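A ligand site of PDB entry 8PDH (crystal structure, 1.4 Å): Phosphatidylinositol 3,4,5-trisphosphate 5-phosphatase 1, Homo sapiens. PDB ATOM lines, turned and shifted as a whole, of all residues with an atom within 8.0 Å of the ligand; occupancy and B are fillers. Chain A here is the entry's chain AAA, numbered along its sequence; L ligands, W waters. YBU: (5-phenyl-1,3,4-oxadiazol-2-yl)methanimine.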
ATOM      1  N   SER A 109      31.449  31.790 -22.837  1.00  0.00           N
ATOM      2  CA  SER A 109      31.357  30.592 -21.969  1.00  0.00           C
ATOM      3  C   SER A 109      30.655  29.463 -22.723  1.00  0.00           C
ATOM      4  O   SER A 109      30.199  29.656 -23.878  1.00  0.00           O
ATOM      5  CB  SER A 109      30.591  30.962 -20.690  1.00  0.00           C
ATOM      6  OG  SER A 109      29.274  31.362 -21.026  1.00  0.00           O
ATOM      7  N   HIS A 110      30.494  28.317 -22.055  1.00  0.00           N
ATOM      8  CA  HIS A 110      29.753  27.146 -22.606  1.00  0.00           C
ATOM      9  C   HIS A 110      30.248  26.813 -24.007  1.00  0.00           C
ATOM     10  O   HIS A 110      29.431  26.698 -24.956  1.00  0.00           O
ATOM     11  CB  HIS A 110      28.251  27.413 -22.624  1.00  0.00           C
ATOM     12  CG  HIS A 110      27.665  27.482 -21.247  1.00  0.00           C
ATOM     13  ND1 HIS A 110      27.458  28.665 -20.589  1.00  0.00           N
ATOM     14  CD2 HIS A 110      27.272  26.511 -20.403  1.00  0.00           C
ATOM     15  CE1 HIS A 110      26.927  28.446 -19.416  1.00  0.00           C
ATOM     16  NE2 HIS A 110      26.794  27.120 -19.291  1.00  0.00           N
ATOM     17  N   ILE A 111      31.562  26.692 -24.151  1.00  0.00           N
ATOM     18  CA  ILE A 111      32.181  26.368 -25.447  1.00  0.00           C
ATOM     19  C   ILE A 111      32.006  24.871 -25.715  1.00  0.00           C
ATOM     20  O   ILE A 111      32.347  24.051 -24.858  1.00  0.00           O
ATOM     21  CB  ILE A 111      33.651  26.812 -25.489  1.00  0.00           C
ATOM     22  CG1 ILE A 111      33.828  28.304 -25.198  1.00  0.00           C
ATOM     23  CG2 ILE A 111      34.311  26.427 -26.805  1.00  0.00           C
ATOM     24  CD1 ILE A 111      35.238  28.660 -24.720  1.00  0.00           C
ATOM     25  N   CYS A 112      31.501  24.552 -26.894  1.00  0.00           N
ATOM     26  CA  CYS A 112      31.234  23.143 -27.336  1.00  0.00           C
ATOM     27  C   CYS A 112      31.862  22.976 -28.729  1.00  0.00           C
ATOM     28  O   CYS A 112      31.885  23.935 -29.532  1.00  0.00           O
ATOM     29  CB  CYS A 112      29.745  22.794 -27.561  1.00  0.00           C
ATOM     30  SG  CYS A 112      28.672  23.389 -26.263  1.00  0.00           S
ATOM     31  N   THR A 113      32.397  21.794 -28.984  1.00  0.00           N
ATOM     32  CA  THR A 113      32.876  21.368 -30.324  1.00  0.00           C
ATOM     33  C   THR A 113      32.277  20.009 -30.629  1.00  0.00           C
ATOM     34  O   THR A 113      32.025  19.232 -29.687  1.00  0.00           O
ATOM     35  CB  THR A 113      34.400  21.277 -30.395  1.00  0.00           C
ATOM     36  OG1 THR A 113      34.900  20.311 -29.494  1.00  0.00           O
ATOM     37  CG2 THR A 113      35.057  22.596 -30.086  1.00  0.00           C
ATOM     38  N   ASP A 114      32.087  19.734 -31.905  1.00  0.00           N
ATOM     39  CA  ASP A 114      31.631  18.396 -32.341  1.00  0.00           C
ATOM     40  C   ASP A 114      31.912  18.233 -33.836  1.00  0.00           C
ATOM     41  O   ASP A 114      32.326  19.181 -34.527  1.00  0.00           O
ATOM     42  CB  ASP A 114      30.149  18.175 -32.061  1.00  0.00           C
ATOM     43  CG  ASP A 114      29.717  16.712 -32.085  1.00  0.00           C
ATOM     44  OD1 ASP A 114      30.589  15.830 -31.837  1.00  0.00           O
ATOM     45  OD2 ASP A 114      28.554  16.463 -32.375  1.00  0.00           O
ATOM     46  N   SER A 133      30.180  25.926 -30.825  1.00  0.00           N
ATOM     47  CA  SER A 133      29.208  26.854 -30.235  1.00  0.00           C
ATOM     48  C   SER A 133      29.708  27.423 -28.935  1.00  0.00           C
ATOM     49  O   SER A 133      30.619  26.867 -28.334  1.00  0.00           O
ATOM     50  CB  SER A 133      27.857  26.210 -30.065  1.00  0.00           C
ATOM     51  OG  SER A 133      27.915  25.234 -29.039  1.00  0.00           O
ATOM     52  N   PHE A 134      29.175  28.580 -28.559  1.00  0.00           N
ATOM     53  CA  PHE A 134      29.414  29.158 -27.249  1.00  0.00           C
ATOM     54  C   PHE A 134      28.352  30.228 -27.012  1.00  0.00           C
ATOM     55  O   PHE A 134      27.605  30.631 -27.914  1.00  0.00           O
ATOM     56  CB  PHE A 134      30.830  29.723 -27.164  1.00  0.00           C
ATOM     57  CG  PHE A 134      31.256  30.673 -28.248  1.00  0.00           C
ATOM     58  CD1 PHE A 134      31.818  30.142 -29.404  1.00  0.00           C
ATOM     59  CD2 PHE A 134      31.124  32.045 -28.148  1.00  0.00           C
ATOM     60  CE1 PHE A 134      32.249  30.955 -30.415  1.00  0.00           C
ATOM     61  CE2 PHE A 134      31.543  32.883 -29.177  1.00  0.00           C
ATOM     62  CZ  PHE A 134      32.105  32.322 -30.336  1.00  0.00           C
ATOM     63  N   MET A 135      28.316  30.686 -25.788  1.00  0.00           N
ATOM     64  CA  MET A 135      27.546  31.870 -25.367  1.00  0.00           C
ATOM     65  C   MET A 135      28.486  33.083 -25.405  1.00  0.00           C
ATOM     66  O   MET A 135      29.619  32.970 -24.963  1.00  0.00           O
ATOM     67  CB  MET A 135      27.047  31.687 -23.932  1.00  0.00           C
ATOM     68  CG  MET A 135      26.011  30.575 -23.732  1.00  0.00           C
ATOM     69  SD  MET A 135      24.455  30.826 -24.579  1.00  0.00           S
ATOM     70  CE  MET A 135      23.975  32.445 -23.968  1.00  0.00           C
ATOM     71  N   THR A 139      23.891  35.770 -25.585  1.00  0.00           N
ATOM     72  CA  THR A 139      23.597  35.373 -26.969  1.00  0.00           C
ATOM     73  C   THR A 139      24.306  34.061 -27.281  1.00  0.00           C
ATOM     74  O   THR A 139      25.523  33.912 -26.946  1.00  0.00           O
ATOM     75  CB  THR A 139      24.022  36.486 -27.924  1.00  0.00           C
ATOM     76  OG1 THR A 139      23.351  37.708 -27.574  1.00  0.00           O
ATOM     77  CG2 THR A 139      23.749  36.130 -29.364  1.00  0.00           C
ATOM     78  N   SER A 140      23.560  33.119 -27.851  1.00  0.00           N
ATOM     79  CA  SER A 140      24.102  31.791 -28.263  1.00  0.00           C
ATOM     80  C   SER A 140      24.532  31.867 -29.743  1.00  0.00           C
ATOM     81  O   SER A 140      23.745  32.334 -30.579  1.00  0.00           O
ATOM     82  CB  SER A 140      23.125  30.701 -28.006  1.00  0.00           C
ATOM     83  OG  SER A 140      21.941  30.942 -28.725  1.00  0.00           O
ATOM     84  N   ALA A 170      26.156  17.835 -32.300  1.00  0.00           N
ATOM     85  CA  ALA A 170      25.737  18.045 -30.895  1.00  0.00           C
ATOM     86  C   ALA A 170      26.395  19.305 -30.384  1.00  0.00           C
ATOM     87  O   ALA A 170      27.546  19.236 -29.938  1.00  0.00           O
ATOM     88  CB  ALA A 170      26.135  16.855 -30.049  1.00  0.00           C
ATOM     89  N   LEU A 171      25.721  20.426 -30.467  1.00  0.00           N
ATOM     90  CA  LEU A 171      26.269  21.708 -29.984  1.00  0.00           C
ATOM     91  C   LEU A 171      25.194  22.417 -29.165  1.00  0.00           C
ATOM     92  O   LEU A 171      24.021  22.015 -29.282  1.00  0.00           O
ATOM     93  CB  LEU A 171      26.654  22.564 -31.186  1.00  0.00           C
ATOM     94  CG  LEU A 171      27.786  22.095 -32.096  1.00  0.00           C
ATOM     95  CD1 LEU A 171      27.806  22.990 -33.336  1.00  0.00           C
ATOM     96  CD2 LEU A 171      29.136  22.103 -31.408  1.00  0.00           C
ATOM     97  N   GLY A 172      25.574  23.444 -28.407  1.00  0.00           N
ATOM     98  CA  GLY A 172      24.606  24.269 -27.664  1.00  0.00           C
ATOM     99  C   GLY A 172      24.077  23.528 -26.464  1.00  0.00           C
ATOM    100  O   GLY A 172      24.668  22.530 -26.004  1.00  0.00           O
ATOM    101  N   ASP A 173      22.958  24.036 -25.981  1.00  0.00           N
ATOM    102  CA  ASP A 173      22.362  23.643 -24.675  1.00  0.00           C
ATOM    103  C   ASP A 173      21.683  22.277 -24.844  1.00  0.00           C
ATOM    104  O   ASP A 173      20.634  22.210 -25.461  1.00  0.00           O
ATOM    105  CB  ASP A 173      21.465  24.773 -24.158  1.00  0.00           C
ATOM    106  CG  ASP A 173      20.843  24.500 -22.812  1.00  0.00           C
ATOM    107  OD1 ASP A 173      21.150  23.418 -22.239  1.00  0.00           O
ATOM    108  OD2 ASP A 173      20.020  25.309 -22.357  1.00  0.00           O
ATOM    109  N   LYS A 174      22.213  21.251 -24.198  1.00  0.00           N
ATOM    110  CA  LYS A 174      21.652  19.871 -24.259  1.00  0.00           C
ATOM    111  C   LYS A 174      20.233  19.835 -23.644  1.00  0.00           C
ATOM    112  O   LYS A 174      19.471  18.860 -23.970  1.00  0.00           O
ATOM    113  CB  LYS A 174      22.596  18.882 -23.563  1.00  0.00           C
ATOM    114  CG  LYS A 174      24.032  18.983 -24.034  1.00  0.00           C
ATOM    115  CD  LYS A 174      24.981  18.003 -23.358  1.00  0.00           C
ATOM    116  CE  LYS A 174      26.419  18.210 -23.788  1.00  0.00           C
ATOM    117  NZ  LYS A 174      27.359  17.475 -22.924  1.00  0.00           N
ATOM    118  N   LYS A 175      19.851  20.816 -22.817  1.00  0.00           N
ATOM    119  CA  LYS A 175      18.474  20.837 -22.241  1.00  0.00           C
ATOM    120  C   LYS A 175      17.468  21.099 -23.353  1.00  0.00           C
ATOM    121  O   LYS A 175      16.270  20.776 -23.166  1.00  0.00           O
ATOM    122  CB  LYS A 175      18.333  21.890 -21.132  1.00  0.00           C
ATOM    123  CG  LYS A 175      19.029  21.478 -19.846  1.00  0.00           C
ATOM    124  CD  LYS A 175      18.990  22.477 -18.717  1.00  0.00           C
ATOM    125  CE  LYS A 175      19.560  21.826 -17.474  1.00  0.00           C
ATOM    126  NZ  LYS A 175      19.678  22.766 -16.340  1.00  0.00           N
ATOM    127  N   LEU A 176      17.936  21.650 -24.497  1.00  0.00           N
ATOM    128  CA  LEU A 176      17.049  21.914 -25.645  1.00  0.00           C
ATOM    129  C   LEU A 176      16.856  20.613 -26.423  1.00  0.00           C
ATOM    130  O   LEU A 176      17.091  20.581 -27.633  1.00  0.00           O
ATOM    131  CB  LEU A 176      17.658  23.042 -26.455  1.00  0.00           C
ATOM    132  CG  LEU A 176      17.775  24.404 -25.764  1.00  0.00           C
ATOM    133  CD1 LEU A 176      18.420  25.427 -26.699  1.00  0.00           C
ATOM    134  CD2 LEU A 176      16.391  24.887 -25.338  1.00  0.00           C
ATOM    135  N   ARG A 184      18.993  25.987 -31.999  1.00  0.00           N
ATOM    136  CA  ARG A 184      19.685  26.134 -30.715  1.00  0.00           C
ATOM    137  C   ARG A 184      20.394  27.473 -30.513  1.00  0.00           C
ATOM    138  O   ARG A 184      20.830  27.744 -29.375  1.00  0.00           O
ATOM    139  CB  ARG A 184      20.606  24.957 -30.414  1.00  0.00           C
ATOM    140  CG  ARG A 184      19.853  23.685 -30.076  1.00  0.00           C
ATOM    141  CD  ARG A 184      20.830  22.608 -29.620  1.00  0.00           C
ATOM    142  NE  ARG A 184      20.102  21.438 -29.185  1.00  0.00           N
ATOM    143  CZ  ARG A 184      20.614  20.399 -28.539  1.00  0.00           C
ATOM    144  NH1 ARG A 184      21.897  20.377 -28.196  1.00  0.00           N
ATOM    145  NH2 ARG A 184      19.808  19.407 -28.226  1.00  0.00           N
ATOM    146  N   PHE A 185      20.558  28.292 -31.549  1.00  0.00           N
ATOM    147  CA  PHE A 185      21.407  29.493 -31.502  1.00  0.00           C
ATOM    148  C   PHE A 185      20.655  30.737 -31.927  1.00  0.00           C
ATOM    149  O   PHE A 185      19.918  30.717 -32.872  1.00  0.00           O
ATOM    150  CB  PHE A 185      22.609  29.264 -32.399  1.00  0.00           C
ATOM    151  CG  PHE A 185      23.306  27.985 -32.031  1.00  0.00           C
ATOM    152  CD1 PHE A 185      23.966  27.885 -30.837  1.00  0.00           C
ATOM    153  CD2 PHE A 185      23.241  26.859 -32.847  1.00  0.00           C
ATOM    154  CE1 PHE A 185      24.556  26.706 -30.411  1.00  0.00           C
ATOM    155  CE2 PHE A 185      23.845  25.684 -32.430  1.00  0.00           C
ATOM    156  CZ  PHE A 185      24.483  25.594 -31.198  1.00  0.00           C
ATOM    157  N   SER A 361      15.535  30.527 -22.412  1.00  0.00           N
ATOM    158  CA  SER A 361      16.411  31.165 -21.397  1.00  0.00           C
ATOM    159  C   SER A 361      15.653  32.070 -20.439  1.00  0.00           C
ATOM    160  O   SER A 361      16.159  32.273 -19.325  1.00  0.00           O
ATOM    161  CB  SER A 361      17.524  31.932 -22.066  1.00  0.00           C
ATOM    162  OG  SER A 361      18.305  31.024 -22.762  1.00  0.00           O
HETATM  163  C1  YBU L   1      28.570  22.212 -25.183  1.00  0.00           C
HETATM  164  C2  YBU L   1      27.483  22.511 -24.263  1.00  0.00           C
HETATM  165  N1  YBU L   1      26.903  21.684 -23.451  1.00  0.00           N
HETATM  166  N2  YBU L   1      25.944  22.412 -22.753  1.00  0.00           N
HETATM  167  C3  YBU L   1      26.026  23.640 -23.177  1.00  0.00           C
HETATM  168  C4  YBU L   1      25.250  24.820 -22.790  1.00  0.00           C
HETATM  169  C5  YBU L   1      25.137  25.896 -23.668  1.00  0.00           C
HETATM  170  C6  YBU L   1      24.412  27.025 -23.304  1.00  0.00           C
HETATM  171  C7  YBU L   1      23.774  27.069 -22.103  1.00  0.00           C
HETATM  172  C8  YBU L   1      23.887  25.994 -21.225  1.00  0.00           C
HETATM  173  C9  YBU L   1      24.610  24.865 -21.559  1.00  0.00           C
HETATM  174  O1  YBU L   1      26.975  23.770 -24.158  1.00  0.00           O
HETATM  175  N3  YBU L   1      29.116  21.024 -25.327  1.00  0.00           N
HETATM  176  O   HOH W   1      32.259  20.058 -26.508  1.00  0.00           O
HETATM  177  O   HOH W   2      28.698  23.791 -21.746  1.00  0.00           O
HETATM  178  O   HOH W   3      22.190  22.977 -19.965  1.00  0.00           O
HETATM  179  O   HOH W   4      24.072  21.235 -21.803  1.00  0.00           O
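Residues that only touch the ligand: His 110, Lys 174, Asp 173 and Met 135.
Hydrophobic or aromatic side chains within 4 Å of the ligand: His 110 and Met 135.
Of the 21 residues printed, 6 come within 4 Å of the ligand.
The nearest printed residue that does not touch the ligand is Ile 111 (4.2 Å).
Water W4 bridges N2 of the ligand and N of Lys 174.
Water W1 lies within hydrogen-bond range of N of Thr 113 (3.0 Å) and N3 of the ligand (3.5 Å).
The side-chain sulfur of Cys 112 sits at hydrogen-bond distance from the backbone NH of Gly 172, 3.8 Å away.
The backbone NH of Cys 112 is in hydrogen-bond range of the backbone carbonyl oxygen of Ser 133 (2.9 Å).
The backbone NH (N) of Gly 172 is in hydrogen-bond range of the side-chain hydroxyl (OG) of Ser 133, at 3.0 Å.
OG of Ser 109 lies within hydrogen-bond range of ND1 of His 110, 3.3 Å away.
OD1 of Asp 173 sits at hydrogen-bond distance from N of Lys 175, 3.0 Å away.
The backbone NH of Met 135 is in hydrogen-bond range of the backbone carbonyl oxygen of Ser 109 (2.9 Å).
The side-chain sulfur of Cys 112 is covalently linked to a carbon (C1) of the ligand, 1.6 Å away.
O of Gly 172 sits close to N1 of the ligand (3.5 Å).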
